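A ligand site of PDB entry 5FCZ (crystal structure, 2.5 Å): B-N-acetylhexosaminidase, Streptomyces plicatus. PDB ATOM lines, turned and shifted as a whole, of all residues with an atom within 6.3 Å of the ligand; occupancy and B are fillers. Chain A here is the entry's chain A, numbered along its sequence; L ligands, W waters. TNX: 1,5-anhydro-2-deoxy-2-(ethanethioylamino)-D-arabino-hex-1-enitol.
The side-chain carboxylate of Glu 450 sits at hydrogen-bond distance from an oxygen (O4) of the ligand, at 2.7 Å.
OD2 of Asp 401 lies within hydrogen-bond range of O6 of the ligand, at 2.7 Å.
An oxygen (O3) of the ligand sits at hydrogen-bond distance from the guanidinium group (NH2) of Arg 168 (2.8 Å).
O6 of the ligand sits at hydrogen-bond distance from NE1 of Trp 414.
OD2 of Asp 319 lies within hydrogen-bond range of N2 of the ligand, at 2.9 Å.
A sulfur (S7) of the ligand lies close to the side-chain hydroxyl of Tyr 399 (3.0 Å).
The side-chain carboxylate (OE1) of Glu 320 lies within hydrogen-bond range of a nitrogen (N2) of the ligand.
OE2 of Glu 450 lies within salt-bridge range of NH1 of Arg 168 (3.5 Å).
The backbone carbonyl oxygen (O) of Asp 401 lies within hydrogen-bond range of the backbone NH (N) of Leu 412 (3.0 Å).
NH2 of Arg 168 lies within salt-bridge range of OD1 of Asp 197 (3.1 Å).
NH1 of Arg 168 lies within salt-bridge range of OD2 of Asp 165, 3.1 Å away.
The side-chain carboxylate (OD2) of Asp 319 sits at hydrogen-bond distance from a ring nitrogen (NE2) of His 256.
OD1 of Asp 319 sits close to OD2 of Asp 252, 2.4 Å away.
A ring nitrogen (NE2) of His 256 is in hydrogen-bond range of the side-chain carboxylate (OE1) of Glu 320 (2.7 Å).
ND1 of His 256 lies within hydrogen-bond range of OD1 of Asp 197.
Merely in contact with the ligand: His 256 (3.1 Å), Trp 350 (3.6 Å), Trp 367 (3.5 Å), Leu 412 (3.5 Å) and Trp 448 (3.3 Å).
Hydrophobic or aromatic side chains within 4 Å of the ligand: His 256, Trp 350, Trp 367, Tyr 399, Leu 412, Trp 414 and Trp 448.
12 residues have an atom within 4 Å of the ligand: Arg 168, His 256, Asp 319, Glu 320, Trp 350, Trp 367, Tyr 399, Asp 401, Leu 412, Trp 414, Trp 448 and Glu 450.
The nearest printed residue that does not touch the ligand is Val 282 (4.1 Å).
Water W2 bridges the side-chain carboxylate (OE2) of Glu 320 and an oxygen (O5) of the ligand.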
ATOM      1  N   ASP A 165       0.720 -28.885  28.413  1.00  0.00           N
ATOM      2  CA  ASP A 165       0.800 -27.971  27.285  1.00  0.00           C
ATOM      3  C   ASP A 165       2.081 -27.166  27.474  1.00  0.00           C
ATOM      4  O   ASP A 165       2.234 -26.429  28.457  1.00  0.00           O
ATOM      5  CB  ASP A 165      -0.480 -27.104  27.257  1.00  0.00           C
ATOM      6  CG  ASP A 165      -0.380 -25.871  26.370  1.00  0.00           C
ATOM      7  OD1 ASP A 165       0.585 -25.743  25.574  1.00  0.00           O
ATOM      8  OD2 ASP A 165      -1.293 -25.013  26.531  1.00  0.00           O
ATOM      9  N   ARG A 168       1.871 -23.116  25.017  1.00  0.00           N
ATOM     10  CA  ARG A 168       1.323 -21.815  25.405  1.00  0.00           C
ATOM     11  C   ARG A 168       2.296 -21.063  26.292  1.00  0.00           C
ATOM     12  O   ARG A 168       2.676 -19.929  25.981  1.00  0.00           O
ATOM     13  CB  ARG A 168      -0.026 -21.982  26.098  1.00  0.00           C
ATOM     14  CG  ARG A 168      -1.133 -21.928  25.130  1.00  0.00           C
ATOM     15  CD  ARG A 168      -0.924 -22.904  23.951  1.00  0.00           C
ATOM     16  NE  ARG A 168      -2.084 -22.851  23.062  1.00  0.00           N
ATOM     17  CZ  ARG A 168      -3.212 -23.516  23.249  1.00  0.00           C
ATOM     18  NH1 ARG A 168      -3.356 -24.376  24.271  1.00  0.00           N
ATOM     19  NH2 ARG A 168      -4.213 -23.328  22.408  1.00  0.00           N
ATOM     20  N   HIS A 194       1.828 -31.636  24.572  1.00  0.00           N
ATOM     21  CA  HIS A 194       1.280 -30.757  23.528  1.00  0.00           C
ATOM     22  C   HIS A 194       2.449 -29.887  23.046  1.00  0.00           C
ATOM     23  O   HIS A 194       2.720 -28.810  23.575  1.00  0.00           O
ATOM     24  CB  HIS A 194       0.111 -29.946  24.086  1.00  0.00           C
ATOM     25  CG  HIS A 194      -0.725 -29.300  23.045  1.00  0.00           C
ATOM     26  ND1 HIS A 194      -1.666 -29.982  22.296  1.00  0.00           N
ATOM     27  CD2 HIS A 194      -0.764 -28.022  22.624  1.00  0.00           C
ATOM     28  CE1 HIS A 194      -2.219 -29.151  21.440  1.00  0.00           C
ATOM     29  NE2 HIS A 194      -1.702 -27.954  21.615  1.00  0.00           N
ATOM     30  N   ASP A 197       1.539 -25.431  18.944  1.00  0.00           N
ATOM     31  CA  ASP A 197       0.260 -24.769  18.873  1.00  0.00           C
ATOM     32  C   ASP A 197       0.465 -23.429  18.171  1.00  0.00           C
ATOM     33  O   ASP A 197       1.453 -23.244  17.454  1.00  0.00           O
ATOM     34  CB  ASP A 197      -0.358 -24.625  20.263  1.00  0.00           C
ATOM     35  CG  ASP A 197      -1.848 -24.596  20.221  1.00  0.00           C
ATOM     36  OD1 ASP A 197      -2.396 -23.531  19.844  1.00  0.00           O
ATOM     37  OD2 ASP A 197      -2.468 -25.627  20.556  1.00  0.00           O
ATOM     38  N   ASP A 252      -0.231 -30.781  16.785  1.00  0.00           N
ATOM     39  CA  ASP A 252      -1.609 -30.490  16.440  1.00  0.00           C
ATOM     40  C   ASP A 252      -1.721 -30.066  14.989  1.00  0.00           C
ATOM     41  O   ASP A 252      -0.980 -29.191  14.526  1.00  0.00           O
ATOM     42  CB  ASP A 252      -2.148 -29.397  17.351  1.00  0.00           C
ATOM     43  CG  ASP A 252      -3.651 -29.441  17.470  1.00  0.00           C
ATOM     44  OD1 ASP A 252      -4.313 -29.991  16.546  1.00  0.00           O
ATOM     45  OD2 ASP A 252      -4.139 -28.927  18.494  1.00  0.00           O
ATOM     46  N   HIS A 256      -4.464 -25.068  15.005  1.00  0.00           N
ATOM     47  CA  HIS A 256      -3.482 -24.772  16.052  1.00  0.00           C
ATOM     48  C   HIS A 256      -2.051 -24.841  15.497  1.00  0.00           C
ATOM     49  O   HIS A 256      -1.131 -25.384  16.108  1.00  0.00           O
ATOM     50  CB  HIS A 256      -3.690 -25.722  17.255  1.00  0.00           C
ATOM     51  CG  HIS A 256      -4.881 -25.366  18.087  1.00  0.00           C
ATOM     52  ND1 HIS A 256      -4.851 -24.389  19.048  1.00  0.00           N
ATOM     53  CD2 HIS A 256      -6.156 -25.839  18.046  1.00  0.00           C
ATOM     54  CE1 HIS A 256      -6.060 -24.277  19.585  1.00  0.00           C
ATOM     55  NE2 HIS A 256      -6.867 -25.145  18.993  1.00  0.00           N
ATOM     56  N   VAL A 282      -8.199 -19.075  19.963  1.00  0.00           N
ATOM     57  CA  VAL A 282      -8.075 -20.312  19.206  1.00  0.00           C
ATOM     58  C   VAL A 282      -8.898 -20.191  17.923  1.00  0.00           C
ATOM     59  O   VAL A 282      -9.793 -19.362  17.809  1.00  0.00           O
ATOM     60  CB  VAL A 282      -8.521 -21.546  20.025  1.00  0.00           C
ATOM     61  CG1 VAL A 282      -7.823 -21.557  21.422  1.00  0.00           C
ATOM     62  CG2 VAL A 282     -10.087 -21.641  20.182  1.00  0.00           C
ATOM     63  N   ASP A 319      -8.134 -30.649  16.720  1.00  0.00           N
ATOM     64  CA  ASP A 319      -9.125 -29.828  17.393  1.00  0.00           C
ATOM     65  C   ASP A 319      -9.182 -28.421  16.800  1.00  0.00           C
ATOM     66  O   ASP A 319      -8.165 -27.858  16.388  1.00  0.00           O
ATOM     67  CB  ASP A 319      -8.790 -29.688  18.874  1.00  0.00           C
ATOM     68  CG  ASP A 319      -7.450 -29.027  19.089  1.00  0.00           C
ATOM     69  OD1 ASP A 319      -6.469 -29.592  18.507  1.00  0.00           O
ATOM     70  OD2 ASP A 319      -7.410 -27.959  19.781  1.00  0.00           O
ATOM     71  N   GLU A 320     -10.394 -27.859  16.798  1.00  0.00           N
ATOM     72  CA  GLU A 320     -10.633 -26.444  16.552  1.00  0.00           C
ATOM     73  C   GLU A 320      -9.951 -25.972  15.282  1.00  0.00           C
ATOM     74  O   GLU A 320      -9.376 -24.877  15.224  1.00  0.00           O
ATOM     75  CB  GLU A 320     -10.220 -25.602  17.758  1.00  0.00           C
ATOM     76  CG  GLU A 320     -10.912 -26.025  19.023  1.00  0.00           C
ATOM     77  CD  GLU A 320     -10.440 -25.216  20.206  1.00  0.00           C
ATOM     78  OE1 GLU A 320      -9.227 -24.903  20.226  1.00  0.00           O
ATOM     79  OE2 GLU A 320     -11.266 -24.913  21.108  1.00  0.00           O
ATOM     80  N   TRP A 350      -7.825 -35.668  18.735  1.00  0.00           N
ATOM     81  CA  TRP A 350      -8.982 -35.176  19.463  1.00  0.00           C
ATOM     82  C   TRP A 350     -10.243 -35.665  18.737  1.00  0.00           C
ATOM     83  O   TRP A 350     -10.181 -36.083  17.581  1.00  0.00           O
ATOM     84  CB  TRP A 350      -8.919 -33.651  19.565  1.00  0.00           C
ATOM     85  CG  TRP A 350      -7.704 -33.125  20.310  1.00  0.00           C
ATOM     86  CD1 TRP A 350      -6.587 -32.509  19.765  1.00  0.00           C
ATOM     87  CD2 TRP A 350      -7.477 -33.170  21.724  1.00  0.00           C
ATOM     88  NE1 TRP A 350      -5.705 -32.169  20.772  1.00  0.00           N
ATOM     89  CE2 TRP A 350      -6.221 -32.576  21.973  1.00  0.00           C
ATOM     90  CE3 TRP A 350      -8.219 -33.657  22.803  1.00  0.00           C
ATOM     91  CZ2 TRP A 350      -5.691 -32.448  23.273  1.00  0.00           C
ATOM     92  CZ3 TRP A 350      -7.699 -33.542  24.086  1.00  0.00           C
ATOM     93  CH2 TRP A 350      -6.451 -32.951  24.307  1.00  0.00           C
ATOM     94  N   GLN A 352     -12.771 -34.552  17.279  1.00  0.00           N
ATOM     95  CA  GLN A 352     -13.088 -34.061  15.941  1.00  0.00           C
ATOM     96  C   GLN A 352     -12.681 -35.051  14.864  1.00  0.00           C
ATOM     97  O   GLN A 352     -13.232 -35.035  13.760  1.00  0.00           O
ATOM     98  CB  GLN A 352     -12.403 -32.716  15.698  1.00  0.00           C
ATOM     99  CG  GLN A 352     -13.067 -31.579  16.407  1.00  0.00           C
ATOM    100  CD  GLN A 352     -12.885 -31.602  17.873  1.00  0.00           C
ATOM    101  OE1 GLN A 352     -11.854 -32.034  18.373  1.00  0.00           O
ATOM    102  NE2 GLN A 352     -13.868 -31.099  18.591  1.00  0.00           N
ATOM    103  N   TRP A 367     -13.167 -34.401  24.351  1.00  0.00           N
ATOM    104  CA  TRP A 367     -13.010 -33.252  25.239  1.00  0.00           C
ATOM    105  C   TRP A 367     -14.288 -32.426  25.311  1.00  0.00           C
ATOM    106  O   TRP A 367     -14.242 -31.256  25.691  1.00  0.00           O
ATOM    107  CB  TRP A 367     -11.831 -32.383  24.807  1.00  0.00           C
ATOM    108  CG  TRP A 367     -11.873 -31.825  23.420  1.00  0.00           C
ATOM    109  CD1 TRP A 367     -11.659 -32.496  22.289  1.00  0.00           C
ATOM    110  CD2 TRP A 367     -12.117 -30.455  23.045  1.00  0.00           C
ATOM    111  NE1 TRP A 367     -11.765 -31.648  21.194  1.00  0.00           N
ATOM    112  CE2 TRP A 367     -12.059 -30.395  21.651  1.00  0.00           C
ATOM    113  CE3 TRP A 367     -12.407 -29.302  23.759  1.00  0.00           C
ATOM    114  CZ2 TRP A 367     -12.257 -29.217  20.944  1.00  0.00           C
ATOM    115  CZ3 TRP A 367     -12.618 -28.136  23.068  1.00  0.00           C
ATOM    116  CH2 TRP A 367     -12.538 -28.099  21.670  1.00  0.00           C
ATOM    117  N   ALA A 395     -14.088 -31.646  29.356  1.00  0.00           N
ATOM    118  CA  ALA A 395     -13.520 -30.347  29.734  1.00  0.00           C
ATOM    119  C   ALA A 395     -14.149 -29.806  30.995  1.00  0.00           C
ATOM    120  O   ALA A 395     -13.546 -28.949  31.670  1.00  0.00           O
ATOM    121  CB  ALA A 395     -13.689 -29.351  28.582  1.00  0.00           C
ATOM    122  N   TYR A 399     -10.147 -31.154  32.951  1.00  0.00           N
ATOM    123  CA  TYR A 399      -9.256 -30.106  32.460  1.00  0.00           C
ATOM    124  C   TYR A 399      -8.718 -29.384  33.679  1.00  0.00           C
ATOM    125  O   TYR A 399      -9.449 -28.650  34.332  1.00  0.00           O
ATOM    126  CB  TYR A 399     -10.001 -29.151  31.536  1.00  0.00           C
ATOM    127  CG  TYR A 399      -9.960 -29.567  30.071  1.00  0.00           C
ATOM    128  CD1 TYR A 399      -9.932 -30.904  29.735  1.00  0.00           C
ATOM    129  CD2 TYR A 399      -9.948 -28.628  29.043  1.00  0.00           C
ATOM    130  CE1 TYR A 399      -9.873 -31.301  28.409  1.00  0.00           C
ATOM    131  CE2 TYR A 399      -9.887 -28.992  27.753  1.00  0.00           C
ATOM    132  CZ  TYR A 399      -9.823 -30.353  27.432  1.00  0.00           C
ATOM    133  OH  TYR A 399      -9.730 -30.804  26.125  1.00  0.00           O
ATOM    134  N   ASP A 401      -6.729 -26.975  33.865  1.00  0.00           N
ATOM    135  CA  ASP A 401      -6.667 -25.528  33.726  1.00  0.00           C
ATOM    136  C   ASP A 401      -7.985 -24.834  34.030  1.00  0.00           C
ATOM    137  O   ASP A 401      -8.001 -23.612  34.052  1.00  0.00           O
ATOM    138  CB  ASP A 401      -6.232 -25.137  32.299  1.00  0.00           C
ATOM    139  CG  ASP A 401      -7.209 -25.620  31.236  1.00  0.00           C
ATOM    140  OD1 ASP A 401      -7.719 -26.763  31.387  1.00  0.00           O
ATOM    141  OD2 ASP A 401      -7.489 -24.859  30.278  1.00  0.00           O
ATOM    142  N   MET A 402      -9.074 -25.573  34.258  1.00  0.00           N
ATOM    143  CA  MET A 402     -10.390 -24.971  34.522  1.00  0.00           C
ATOM    144  C   MET A 402     -10.503 -24.513  35.982  1.00  0.00           C
ATOM    145  O   MET A 402     -10.186 -25.277  36.908  1.00  0.00           O
ATOM    146  CB  MET A 402     -11.510 -25.964  34.198  1.00  0.00           C
ATOM    147  CG  MET A 402     -12.722 -25.300  33.590  1.00  0.00           C
ATOM    148  SD  MET A 402     -12.381 -24.538  31.967  1.00  0.00           S
ATOM    149  CE  MET A 402     -11.751 -25.903  30.954  1.00  0.00           C
ATOM    150  N   LEU A 412      -9.069 -20.970  33.235  1.00  0.00           N
ATOM    151  CA  LEU A 412     -10.174 -20.573  32.373  1.00  0.00           C
ATOM    152  C   LEU A 412     -11.514 -21.027  32.938  1.00  0.00           C
ATOM    153  O   LEU A 412     -11.592 -21.782  33.915  1.00  0.00           O
ATOM    154  CB  LEU A 412      -9.975 -21.132  30.966  1.00  0.00           C
ATOM    155  CG  LEU A 412      -8.653 -20.765  30.262  1.00  0.00           C
ATOM    156  CD1 LEU A 412      -8.568 -21.412  28.849  1.00  0.00           C
ATOM    157  CD2 LEU A 412      -8.493 -19.296  30.154  1.00  0.00           C
ATOM    158  N   TRP A 414     -14.359 -21.327  30.362  1.00  0.00           N
ATOM    159  CA  TRP A 414     -15.249 -21.540  29.233  1.00  0.00           C
ATOM    160  C   TRP A 414     -16.081 -22.806  29.402  1.00  0.00           C
ATOM    161  O   TRP A 414     -17.155 -22.920  28.818  1.00  0.00           O
ATOM    162  CB  TRP A 414     -14.423 -21.589  27.947  1.00  0.00           C
ATOM    163  CG  TRP A 414     -13.525 -22.784  27.767  1.00  0.00           C
ATOM    164  CD1 TRP A 414     -12.197 -22.847  28.040  1.00  0.00           C
ATOM    165  CD2 TRP A 414     -13.881 -24.079  27.254  1.00  0.00           C
ATOM    166  NE1 TRP A 414     -11.698 -24.095  27.723  1.00  0.00           N
ATOM    167  CE2 TRP A 414     -12.711 -24.875  27.240  1.00  0.00           C
ATOM    168  CE3 TRP A 414     -15.075 -24.645  26.803  1.00  0.00           C
ATOM    169  CZ2 TRP A 414     -12.702 -26.200  26.793  1.00  0.00           C
ATOM    170  CZ3 TRP A 414     -15.063 -25.962  26.354  1.00  0.00           C
ATOM    171  CH2 TRP A 414     -13.875 -26.728  26.352  1.00  0.00           C
ATOM    172  N   TRP A 448      -3.738 -27.298  30.312  1.00  0.00           N
ATOM    173  CA  TRP A 448      -3.389 -26.273  29.321  1.00  0.00           C
ATOM    174  C   TRP A 448      -2.779 -25.066  30.004  1.00  0.00           C
ATOM    175  O   TRP A 448      -3.066 -24.781  31.172  1.00  0.00           O
ATOM    176  CB  TRP A 448      -4.641 -25.857  28.530  1.00  0.00           C
ATOM    177  CG  TRP A 448      -5.311 -27.010  27.867  1.00  0.00           C
ATOM    178  CD1 TRP A 448      -6.341 -27.724  28.359  1.00  0.00           C
ATOM    179  CD2 TRP A 448      -4.974 -27.588  26.612  1.00  0.00           C
ATOM    180  NE1 TRP A 448      -6.674 -28.733  27.491  1.00  0.00           N
ATOM    181  CE2 TRP A 448      -5.852 -28.669  26.399  1.00  0.00           C
ATOM    182  CE3 TRP A 448      -3.994 -27.305  25.631  1.00  0.00           C
ATOM    183  CZ2 TRP A 448      -5.809 -29.463  25.241  1.00  0.00           C
ATOM    184  CZ3 TRP A 448      -3.954 -28.091  24.494  1.00  0.00           C
ATOM    185  CH2 TRP A 448      -4.860 -29.144  24.295  1.00  0.00           C
ATOM    186  N   THR A 449      -1.892 -24.360  29.293  1.00  0.00           N
ATOM    187  CA  THR A 449      -1.109 -23.324  29.962  1.00  0.00           C
ATOM    188  C   THR A 449      -1.301 -21.898  29.385  1.00  0.00           C
ATOM    189  O   THR A 449      -0.408 -21.064  29.504  1.00  0.00           O
ATOM    190  CB  THR A 449       0.363 -23.745  29.994  1.00  0.00           C
ATOM    191  OG1 THR A 449       0.871 -23.978  28.670  1.00  0.00           O
ATOM    192  CG2 THR A 449       0.513 -25.012  30.791  1.00  0.00           C
ATOM    193  N   GLU A 450      -2.483 -21.545  28.846  1.00  0.00           N
ATOM    194  CA  GLU A 450      -2.712 -20.130  28.492  1.00  0.00           C
ATOM    195  C   GLU A 450      -2.379 -19.199  29.646  1.00  0.00           C
ATOM    196  O   GLU A 450      -1.867 -18.096  29.437  1.00  0.00           O
ATOM    197  CB  GLU A 450      -4.152 -19.858  28.062  1.00  0.00           C
ATOM    198  CG  GLU A 450      -4.461 -20.271  26.657  1.00  0.00           C
ATOM    199  CD  GLU A 450      -4.936 -21.719  26.580  1.00  0.00           C
ATOM    200  OE1 GLU A 450      -4.680 -22.519  27.519  1.00  0.00           O
ATOM    201  OE2 GLU A 450      -5.582 -22.042  25.564  1.00  0.00           O
HETATM  202  C1  TNX L   1      -9.447 -25.656  23.855  1.00  0.00           C
HETATM  203  S7  TNX L   1      -9.177 -28.334  24.606  1.00  0.00           S
HETATM  204  C2  TNX L   1      -8.400 -26.168  23.246  1.00  0.00           C
HETATM  205  C3  TNX L   1      -6.992 -25.729  23.663  1.00  0.00           C
HETATM  206  C4  TNX L   1      -7.171 -24.801  24.882  1.00  0.00           C
HETATM  207  C5  TNX L   1      -8.219 -25.396  25.856  1.00  0.00           C
HETATM  208  C6  TNX L   1      -8.487 -24.399  26.976  1.00  0.00           C
HETATM  209  C7  TNX L   1      -8.738 -28.447  23.000  1.00  0.00           C
HETATM  210  C8  TNX L   1      -8.510 -29.785  22.332  1.00  0.00           C
HETATM  211  N2  TNX L   1      -8.556 -27.293  22.364  1.00  0.00           N
HETATM  212  O3  TNX L   1      -6.331 -25.136  22.592  1.00  0.00           O
HETATM  213  O4  TNX L   1      -5.939 -24.673  25.524  1.00  0.00           O
HETATM  214  O5  TNX L   1      -9.492 -25.652  25.215  1.00  0.00           O
HETATM  215  O6  TNX L   1      -9.003 -25.081  28.081  1.00  0.00           O
HETATM  216  O   HOH W   1      -5.141 -27.028  21.231  1.00  0.00           O
HETATM  217  O   HOH W   2     -11.469 -23.596  23.519  1.00  0.00           O
